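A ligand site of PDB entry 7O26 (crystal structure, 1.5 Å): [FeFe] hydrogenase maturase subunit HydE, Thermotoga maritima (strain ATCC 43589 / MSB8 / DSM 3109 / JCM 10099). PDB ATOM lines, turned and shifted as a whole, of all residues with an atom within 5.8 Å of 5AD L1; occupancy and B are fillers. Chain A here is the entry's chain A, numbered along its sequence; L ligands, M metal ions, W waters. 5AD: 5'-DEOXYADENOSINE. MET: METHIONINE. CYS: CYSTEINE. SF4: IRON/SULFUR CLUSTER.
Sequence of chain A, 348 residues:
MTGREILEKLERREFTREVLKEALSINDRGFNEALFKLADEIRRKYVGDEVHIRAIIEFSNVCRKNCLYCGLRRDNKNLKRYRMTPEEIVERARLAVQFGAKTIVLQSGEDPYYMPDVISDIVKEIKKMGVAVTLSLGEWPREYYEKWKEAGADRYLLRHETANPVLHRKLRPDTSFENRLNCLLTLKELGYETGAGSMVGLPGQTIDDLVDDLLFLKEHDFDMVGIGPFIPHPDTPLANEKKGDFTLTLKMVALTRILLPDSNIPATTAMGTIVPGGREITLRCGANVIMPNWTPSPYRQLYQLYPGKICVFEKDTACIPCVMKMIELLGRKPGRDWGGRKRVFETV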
ATOM      1  N   TYR A  69      14.919   5.399   8.405  1.00  0.00           N
ATOM      2  CA  TYR A  69      13.489   5.258   8.170  1.00  0.00           C
ATOM      3  C   TYR A  69      12.660   5.242   9.456  1.00  0.00           C
ATOM      4  O   TYR A  69      11.431   5.408   9.385  1.00  0.00           O
ATOM      5  CB  TYR A  69      13.211   3.937   7.417  1.00  0.00           C
ATOM      6  CG  TYR A  69      13.988   2.739   7.938  1.00  0.00           C
ATOM      7  CD1 TYR A  69      13.557   2.010   9.041  1.00  0.00           C
ATOM      8  CD2 TYR A  69      15.189   2.342   7.320  1.00  0.00           C
ATOM      9  CE1 TYR A  69      14.282   0.918   9.525  1.00  0.00           C
ATOM     10  CE2 TYR A  69      15.899   1.241   7.790  1.00  0.00           C
ATOM     11  CZ  TYR A  69      15.452   0.550   8.892  1.00  0.00           C
ATOM     12  OH  TYR A  69      16.156  -0.535   9.365  1.00  0.00           O
ATOM     13  N   CYS A  70      13.274   5.024  10.617  1.00  0.00           N
ATOM     14  CA  CYS A  70      12.551   4.621  11.810  1.00  0.00           C
ATOM     15  C   CYS A  70      12.280   5.797  12.739  1.00  0.00           C
ATOM     16  O   CYS A  70      13.221   6.535  13.095  1.00  0.00           O
ATOM     17  CB  CYS A  70      13.369   3.579  12.557  1.00  0.00           C
ATOM     18  SG  CYS A  70      12.525   2.934  13.986  1.00  0.00           S
ATOM     19  N   GLY A  71      11.026   5.943  13.184  1.00  0.00           N
ATOM     20  CA  GLY A  71      10.674   6.999  14.128  1.00  0.00           C
ATOM     21  C   GLY A  71      11.313   6.867  15.522  1.00  0.00           C
ATOM     22  O   GLY A  71      11.314   7.850  16.271  1.00  0.00           O
ATOM     23  N   GLN A 107       9.147  -6.970  21.659  1.00  0.00           N
ATOM     24  CA  GLN A 107       9.879  -6.156  20.700  1.00  0.00           C
ATOM     25  C   GLN A 107      10.258  -4.826  21.331  1.00  0.00           C
ATOM     26  O   GLN A 107       9.488  -4.264  22.117  1.00  0.00           O
ATOM     27  CB  GLN A 107       9.047  -5.910  19.417  1.00  0.00           C
ATOM     28  CG  GLN A 107       9.857  -5.252  18.307  1.00  0.00           C
ATOM     29  CD  GLN A 107       9.054  -4.987  17.051  1.00  0.00           C
ATOM     30  OE1 GLN A 107       8.322  -4.020  16.969  1.00  0.00           O
ATOM     31  NE2 GLN A 107       9.207  -5.852  16.056  1.00  0.00           N
ATOM     32  N   SER A 136      12.433  -9.798  19.523  1.00  0.00           N
ATOM     33  CA  SER A 136      12.709  -8.924  18.374  1.00  0.00           C
ATOM     34  C   SER A 136      13.327  -7.667  18.963  1.00  0.00           C
ATOM     35  O   SER A 136      12.685  -6.644  19.107  1.00  0.00           O
ATOM     36  CB  SER A 136      11.400  -8.616  17.651  1.00  0.00           C
ATOM     37  OG  SER A 136      11.593  -7.880  16.473  1.00  0.00           O
ATOM     38  N   ARG A 159      14.332  -8.692  10.959  1.00  0.00           N
ATOM     39  CA  ARG A 159      14.108  -8.442   9.544  1.00  0.00           C
ATOM     40  C   ARG A 159      15.399  -7.970   8.891  1.00  0.00           C
ATOM     41  O   ARG A 159      16.132  -7.154   9.434  1.00  0.00           O
ATOM     42  CB  ARG A 159      12.954  -7.469   9.364  1.00  0.00           C
ATOM     43  CG  ARG A 159      11.621  -8.106   9.811  1.00  0.00           C
ATOM     44  CD  ARG A 159      10.432  -7.136   9.924  1.00  0.00           C
ATOM     45  NE  ARG A 159      10.003  -6.607   8.623  1.00  0.00           N
ATOM     46  CZ  ARG A 159       9.050  -5.694   8.463  1.00  0.00           C
ATOM     47  NH1 ARG A 159       8.417  -5.176   9.506  1.00  0.00           N
ATOM     48  NH2 ARG A 159       8.751  -5.268   7.242  1.00  0.00           N
ATOM     49  N   GLU A 161      15.697  -6.220   6.266  1.00  0.00           N
ATOM     50  CA  GLU A 161      15.398  -4.848   5.823  1.00  0.00           C
ATOM     51  C   GLU A 161      15.622  -4.664   4.338  1.00  0.00           C
ATOM     52  O   GLU A 161      14.699  -4.274   3.606  1.00  0.00           O
ATOM     53  CB  GLU A 161      16.161  -3.770   6.633  1.00  0.00           C
ATOM     54  CG  GLU A 161      16.174  -4.036   8.156  1.00  0.00           C
ATOM     55  CD  GLU A 161      14.783  -3.987   8.827  1.00  0.00           C
ATOM     56  OE1 GLU A 161      13.734  -3.966   8.152  1.00  0.00           O
ATOM     57  OE2 GLU A 161      14.754  -3.972  10.084  1.00  0.00           O
ATOM     58  N   ARG A 180      24.047  -7.777   9.872  1.00  0.00           N
ATOM     59  CA  ARG A 180      22.675  -8.280   9.968  1.00  0.00           C
ATOM     60  C   ARG A 180      22.611  -9.750   9.583  1.00  0.00           C
ATOM     61  O   ARG A 180      21.945 -10.544  10.247  1.00  0.00           O
ATOM     62  CB  ARG A 180      21.750  -7.480   9.030  1.00  0.00           C
ATOM     63  CG  ARG A 180      20.233  -7.578   9.357  1.00  0.00           C
ATOM     64  CD  ARG A 180      19.910  -6.715  10.565  1.00  0.00           C
ATOM     65  NE  ARG A 180      18.466  -6.568  10.789  1.00  0.00           N
ATOM     66  CZ  ARG A 180      17.944  -5.880  11.801  1.00  0.00           C
ATOM     67  NH1 ARG A 180      18.763  -5.281  12.685  1.00  0.00           N
ATOM     68  NH2 ARG A 180      16.625  -5.775  11.917  1.00  0.00           N
ATOM     69  N   GLY A 197      13.080 -10.809   6.529  1.00  0.00           N
ATOM     70  CA  GLY A 197      12.057 -10.053   5.811  1.00  0.00           C
ATOM     71  C   GLY A 197      12.473  -8.604   5.570  1.00  0.00           C
ATOM     72  O   GLY A 197      13.397  -8.119   6.223  1.00  0.00           O
ATOM     73  N   SER A 198      11.816  -7.916   4.655  1.00  0.00           N
ATOM     74  CA  SER A 198      12.341  -6.634   4.178  1.00  0.00           C
ATOM     75  C   SER A 198      11.201  -5.623   4.095  1.00  0.00           C
ATOM     76  O   SER A 198      10.023  -5.968   4.230  1.00  0.00           O
ATOM     77  CB  SER A 198      12.994  -6.801   2.820  1.00  0.00           C
ATOM     78  OG  SER A 198      12.140  -7.553   1.954  1.00  0.00           O
ATOM     79  N   MET A 199      11.560  -4.366   3.908  1.00  0.00           N
ATOM     80  CA  MET A 199      10.561  -3.373   3.554  1.00  0.00           C
ATOM     81  C   MET A 199      10.549  -3.201   2.036  1.00  0.00           C
ATOM     82  O   MET A 199      11.557  -3.446   1.359  1.00  0.00           O
ATOM     83  CB  MET A 199      10.887  -2.039   4.233  1.00  0.00           C
ATOM     84  CG  MET A 199      10.669  -2.033   5.778  1.00  0.00           C
ATOM     85  SD  MET A 199      11.305  -0.499   6.537  1.00  0.00           S
ATOM     86  CE  MET A 199      13.045  -0.864   6.502  1.00  0.00           C
ATOM     87  N   GLY A 228       6.633  -5.648   4.716  1.00  0.00           N
ATOM     88  CA  GLY A 228       5.689  -4.555   4.720  1.00  0.00           C
ATOM     89  C   GLY A 228       6.210  -3.399   3.891  1.00  0.00           C
ATOM     90  O   GLY A 228       7.400  -3.326   3.557  1.00  0.00           O
ATOM     91  N   PRO A 229       5.325  -2.466   3.550  1.00  0.00           N
ATOM     92  CA  PRO A 229       5.757  -1.281   2.796  1.00  0.00           C
ATOM     93  C   PRO A 229       6.501  -0.319   3.691  1.00  0.00           C
ATOM     94  O   PRO A 229       6.208  -0.213   4.875  1.00  0.00           O
ATOM     95  CB  PRO A 229       4.424  -0.650   2.380  1.00  0.00           C
ATOM     96  CG  PRO A 229       3.491  -1.003   3.594  1.00  0.00           C
ATOM     97  CD  PRO A 229       3.954  -2.367   4.051  1.00  0.00           C
ATOM     98  N   PHE A 230       7.457   0.394   3.094  1.00  0.00           N
ATOM     99  CA  PHE A 230       8.030   1.563   3.775  1.00  0.00           C
ATOM    100  C   PHE A 230       6.983   2.671   3.938  1.00  0.00           C
ATOM    101  O   PHE A 230       6.311   3.049   2.980  1.00  0.00           O
ATOM    102  CB  PHE A 230       9.207   2.082   2.940  1.00  0.00           C
ATOM    103  CG  PHE A 230       9.637   3.475   3.322  1.00  0.00           C
ATOM    104  CD1 PHE A 230      10.182   3.732   4.585  1.00  0.00           C
ATOM    105  CD2 PHE A 230       9.522   4.505   2.417  1.00  0.00           C
ATOM    106  CE1 PHE A 230      10.583   5.036   4.920  1.00  0.00           C
ATOM    107  CE2 PHE A 230       9.931   5.797   2.766  1.00  0.00           C
ATOM    108  CZ  PHE A 230      10.448   6.038   4.019  1.00  0.00           C
ATOM    109  N   ILE A 231       6.870   3.212   5.150  1.00  0.00           N
ATOM    110  CA  ILE A 231       5.951   4.311   5.449  1.00  0.00           C
ATOM    111  C   ILE A 231       6.767   5.476   5.987  1.00  0.00           C
ATOM    112  O   ILE A 231       7.365   5.362   7.058  1.00  0.00           O
ATOM    113  CB  ILE A 231       4.874   3.892   6.457  1.00  0.00           C
ATOM    114  CG1 ILE A 231       4.087   2.671   5.911  1.00  0.00           C
ATOM    115  CG2 ILE A 231       3.937   5.039   6.764  1.00  0.00           C
ATOM    116  CD1 ILE A 231       3.172   2.020   6.943  1.00  0.00           C
ATOM    117  N   PRO A 232       6.843   6.612   5.296  1.00  0.00           N
ATOM    118  CA  PRO A 232       7.693   7.700   5.777  1.00  0.00           C
ATOM    119  C   PRO A 232       7.181   8.291   7.074  1.00  0.00           C
ATOM    120  O   PRO A 232       5.966   8.438   7.281  1.00  0.00           O
ATOM    121  CB  PRO A 232       7.632   8.739   4.648  1.00  0.00           C
ATOM    122  CG  PRO A 232       6.358   8.415   3.905  1.00  0.00           C
ATOM    123  CD  PRO A 232       6.147   6.937   4.031  1.00  0.00           C
ATOM    124  N   HIS A 233       8.121   8.649   7.953  1.00  0.00           N
ATOM    125  CA  HIS A 233       7.855   9.216   9.262  1.00  0.00           C
ATOM    126  C   HIS A 233       8.320  10.654   9.257  1.00  0.00           C
ATOM    127  O   HIS A 233       9.466  10.925   8.874  1.00  0.00           O
ATOM    128  CB  HIS A 233       8.601   8.424  10.352  1.00  0.00           C
ATOM    129  CG  HIS A 233       8.186   8.795  11.751  1.00  0.00           C
ATOM    130  ND1 HIS A 233       8.339  10.063  12.269  1.00  0.00           N
ATOM    131  CD2 HIS A 233       7.617   8.050  12.732  1.00  0.00           C
ATOM    132  CE1 HIS A 233       7.887  10.089  13.504  1.00  0.00           C
ATOM    133  NE2 HIS A 233       7.448   8.887  13.814  1.00  0.00           N
ATOM    134  N   ALA A 270       2.084  -2.887   9.138  1.00  0.00           N
ATOM    135  CA  ALA A 270       2.269  -1.866   8.096  1.00  0.00           C
ATOM    136  C   ALA A 270       1.308  -2.095   6.938  1.00  0.00           C
ATOM    137  O   ALA A 270       0.810  -1.134   6.325  1.00  0.00           O
ATOM    138  CB  ALA A 270       3.712  -1.843   7.616  1.00  0.00           C
ATOM    139  N   TYR A 303       5.039   4.146  20.478  1.00  0.00           N
ATOM    140  CA  TYR A 303       5.883   3.245  19.716  1.00  0.00           C
ATOM    141  C   TYR A 303       5.591   3.494  18.238  1.00  0.00           C
ATOM    142  O   TYR A 303       4.871   2.759  17.585  1.00  0.00           O
ATOM    143  CB  TYR A 303       5.634   1.821  20.157  1.00  0.00           C
ATOM    144  CG  TYR A 303       6.685   0.834  19.748  1.00  0.00           C
ATOM    145  CD1 TYR A 303       7.810   0.638  20.546  1.00  0.00           C
ATOM    146  CD2 TYR A 303       6.525   0.072  18.618  1.00  0.00           C
ATOM    147  CE1 TYR A 303       8.761  -0.303  20.193  1.00  0.00           C
ATOM    148  CE2 TYR A 303       7.471  -0.877  18.262  1.00  0.00           C
ATOM    149  CZ  TYR A 303       8.587  -1.037  19.052  1.00  0.00           C
ATOM    150  OH  TYR A 303       9.516  -1.995  18.712  1.00  0.00           O
ATOM    151  N   LEU A 305       7.029   3.611  15.014  1.00  0.00           N
ATOM    152  CA  LEU A 305       7.983   3.290  13.955  1.00  0.00           C
ATOM    153  C   LEU A 305       7.677   4.094  12.692  1.00  0.00           C
ATOM    154  O   LEU A 305       8.582   4.640  12.052  1.00  0.00           O
ATOM    155  CB  LEU A 305       7.940   1.793  13.651  1.00  0.00           C
ATOM    156  CG  LEU A 305       8.238   0.827  14.793  1.00  0.00           C
ATOM    157  CD1 LEU A 305       8.014  -0.582  14.293  1.00  0.00           C
ATOM    158  CD2 LEU A 305       9.647   0.956  15.261  1.00  0.00           C
ATOM    159  N   TYR A 306       6.412   4.143  12.324  1.00  0.00           N
ATOM    160  CA  TYR A 306       5.886   4.949  11.233  1.00  0.00           C
ATOM    161  C   TYR A 306       4.571   5.538  11.722  1.00  0.00           C
ATOM    162  O   TYR A 306       3.968   5.006  12.662  1.00  0.00           O
ATOM    163  CB  TYR A 306       5.615   4.077   9.999  1.00  0.00           C
ATOM    164  CG  TYR A 306       5.011   2.712  10.321  1.00  0.00           C
ATOM    165  CD1 TYR A 306       3.647   2.550  10.519  1.00  0.00           C
ATOM    166  CD2 TYR A 306       5.825   1.596  10.428  1.00  0.00           C
ATOM    167  CE1 TYR A 306       3.107   1.306  10.821  1.00  0.00           C
ATOM    168  CE2 TYR A 306       5.306   0.368  10.718  1.00  0.00           C
ATOM    169  CZ  TYR A 306       3.941   0.216  10.926  1.00  0.00           C
ATOM    170  OH  TYR A 306       3.419  -1.016  11.229  1.00  0.00           O
HETATM  171  N1  5AD L   1       8.023   1.921   7.567  1.00  0.00           N
HETATM  172  C2  5AD L   1       7.755   0.602   7.488  1.00  0.00           C
HETATM  173  N3  5AD L   1       8.331  -0.276   8.286  1.00  0.00           N
HETATM  174  C4  5AD L   1       9.248   0.150   9.223  1.00  0.00           C
HETATM  175  N9  5AD L   1       9.984  -0.503  10.138  1.00  0.00           N
HETATM  176  C8  5AD L   1      10.742   0.379  10.811  1.00  0.00           C
HETATM  177  N7  5AD L   1      10.485   1.606  10.362  1.00  0.00           N
HETATM  178  C5  5AD L   1       9.561   1.473   9.337  1.00  0.00           C
HETATM  179  C6  5AD L   1       8.897   2.394   8.468  1.00  0.00           C
HETATM  180  N6  5AD L   1       9.163   3.818   8.552  1.00  0.00           N
HETATM  181  C1' 5AD L   1       9.995  -1.847  10.281  1.00  0.00           C
HETATM  182  C2' 5AD L   1      11.437  -2.477  10.145  1.00  0.00           C
HETATM  183  C3' 5AD L   1      11.705  -2.949  11.284  1.00  0.00           C
HETATM  184  C4' 5AD L   1      10.215  -3.305  11.850  1.00  0.00           C
HETATM  185  C5' 5AD L   1      10.245  -3.563  13.327  1.00  0.00           C
HETATM  186  O4' 5AD L   1       9.587  -2.216  11.654  1.00  0.00           O
HETATM  187  O2' 5AD L   1      11.404  -3.507   9.027  1.00  0.00           O
HETATM  188  O3' 5AD L   1      12.558  -4.173  11.335  1.00  0.00           O
HETATM  189  N   MET L   2      15.084  -2.700  17.113  1.00  0.00           N
HETATM  190  CA  MET L   2      14.842  -4.019  16.558  1.00  0.00           C
HETATM  191  C   MET L   2      15.234  -4.072  15.074  1.00  0.00           C
HETATM  192  O   MET L   2      15.430  -5.167  14.517  1.00  0.00           O
HETATM  193  CB  MET L   2      13.378  -4.402  16.738  1.00  0.00           C
HETATM  194  CG  MET L   2      12.499  -3.933  15.616  1.00  0.00           C
HETATM  195  SD  MET L   2      12.444  -2.142  15.251  1.00  0.00           S
HETATM  196  CE  MET L   2      11.566  -1.606  16.697  1.00  0.00           C
HETATM  197  OXT MET L   2      15.370  -3.031  14.410  1.00  0.00           O
HETATM  198  N   CYS L   3       4.898  -5.051  13.693  1.00  0.00           N
HETATM  199  CA  CYS L   3       5.379  -3.962  12.843  1.00  0.00           C
HETATM  200  C   CYS L   3       5.030  -4.311  11.415  1.00  0.00           C
HETATM  201  O   CYS L   3       5.090  -5.488  11.111  1.00  0.00           O
HETATM  202  CB  CYS L   3       6.890  -3.862  12.982  1.00  0.00           C
HETATM  203  SG  CYS L   3       7.673  -5.505  12.796  1.00  0.00           S
HETATM  204  OXT CYS L   3       4.680  -3.487  10.584  1.00  0.00           O
HETATM  205 FE1  SF4 L   4      14.222   1.638  14.714  1.00  0.00          FE
HETATM  206 FE2  SF4 L   4      16.255   1.264  16.464  1.00  0.00          FE
HETATM  207 FE3  SF4 L   4      16.648   0.875  13.780  1.00  0.00          FE
HETATM  208 FE4  SF4 L   4      15.016  -0.986  15.259  1.00  0.00          FE
HETATM  209  S1  SF4 L   4      17.288  -0.518  15.466  1.00  0.00           S
HETATM  210  S2  SF4 L   4      14.621  -0.027  13.187  1.00  0.00           S
HETATM  211  S3  SF4 L   4      14.081   0.557  16.716  1.00  0.00           S
HETATM  212  S4  SF4 L   4      16.159   2.860  14.828  1.00  0.00           S
HETATM  213 FE    FE M   1       5.776  -6.674  12.676  1.00  0.00          FE
HETATM  214  O   HOH W   1       7.131  -2.821   7.699  1.00  0.00           O
HETATM  215  O   HOH W   2      13.227  -6.562  12.863  1.00  0.00           O
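An iron atom (FE1) of SF4 L4 is bound by the side-chain sulfur (SG) of Cys 70 (2.3 Å).
O of Tyr 69 sits at hydrogen-bond distance from N6 of 5AD L1 (2.9 Å).
OH of Tyr 306 sits at hydrogen-bond distance from OXT of CYS L3, 2.8 Å away.
The backbone carbonyl oxygen (O) of Ile 231 sits at hydrogen-bond distance from a nitrogen (N6) of 5AD L1 (2.8 Å).
OXT of CYS L3 is in hydrogen-bond range of N of Ala 270, 3.0 Å away.
The guanidinium group of Arg 180 lies within salt-bridge range of an oxygen (O) of MET L2, 2.9 Å away.
NE of Arg 159 sits close to O2' of 5AD L1.
The side-chain amide nitrogen (NE2) of Gln 107 sits close to a sulfur (SG) of CYS L3 (3.6 Å).
A sulfur (SG) of CYS L3 sits close to the guanidinium group (NH1) of Arg 159.
OE1 of Glu 161 lies within hydrogen-bond range of O2' of 5AD L1.
N1 of 5AD L1 is in hydrogen-bond range of N of Ile 231.
An oxygen (OXT) of MET L2 is bound to an iron atom (FE4) of SF4 L4, at 2.2 Å.
The side-chain amide oxygen of Gln 107 is in hydrogen-bond range of the side-chain hydroxyl of Tyr 303 (2.9 Å).
OE2 of Glu 161 is in salt-bridge range of NH2 of Arg 180 (3.2 Å).
N of Ala 270 sits at hydrogen-bond distance from OH of Tyr 306, at 3.1 Å.
The backbone carbonyl oxygen of Ser 198 sits at hydrogen-bond distance from the guanidinium group of Arg 159 (3.3 Å).
O of Glu 161 is in hydrogen-bond range of N of Met 199 (3.2 Å).
The guanidinium group (NE) of Arg 180 sits at hydrogen-bond distance from the backbone carbonyl oxygen (O) of Arg 159.
NE2 of Gln 107 is in hydrogen-bond range of OG of Ser 136 (3.2 Å).
The backbone carbonyl oxygen (O) of Gly 197 sits at hydrogen-bond distance from the backbone NH (N) of Glu 161.
N3 of 5AD L1 lies close to SD of Met 199 (3.5 Å).
Cys 70 touches 5AD L1.
Gln 107 touches 5AD L1.
Pro 229 touches 5AD L1 (O to C2, 3.1 Å).
Phe 230 touches 5AD L1.
Leu 305 touches 5AD L1.
Tyr 306 touches 5AD L1 (CD2 to N1, 3.6 Å).
Hydrophobic or aromatic side chains within 4 Å of 5AD L1: Tyr 69, Met 199, Ile 231, Leu 305 and Tyr 306.
Of the 21 residues printed, 11 come within 4 Å of 5AD L1.
The nearest printed residue that does not touch 5AD L1 is Arg 180 (4.4 Å).
Water W1 lies within hydrogen-bond range of a nitrogen (N3) of 5AD L1 and the guanidinium group of Arg 159.
Water W2 lies within hydrogen-bond range of an oxygen (O3') of 5AD L1 (2.9 Å), the backbone NH (N) of Arg 159 (3.1 Å) and an oxygen (O) of MET L2 (3.1 Å).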
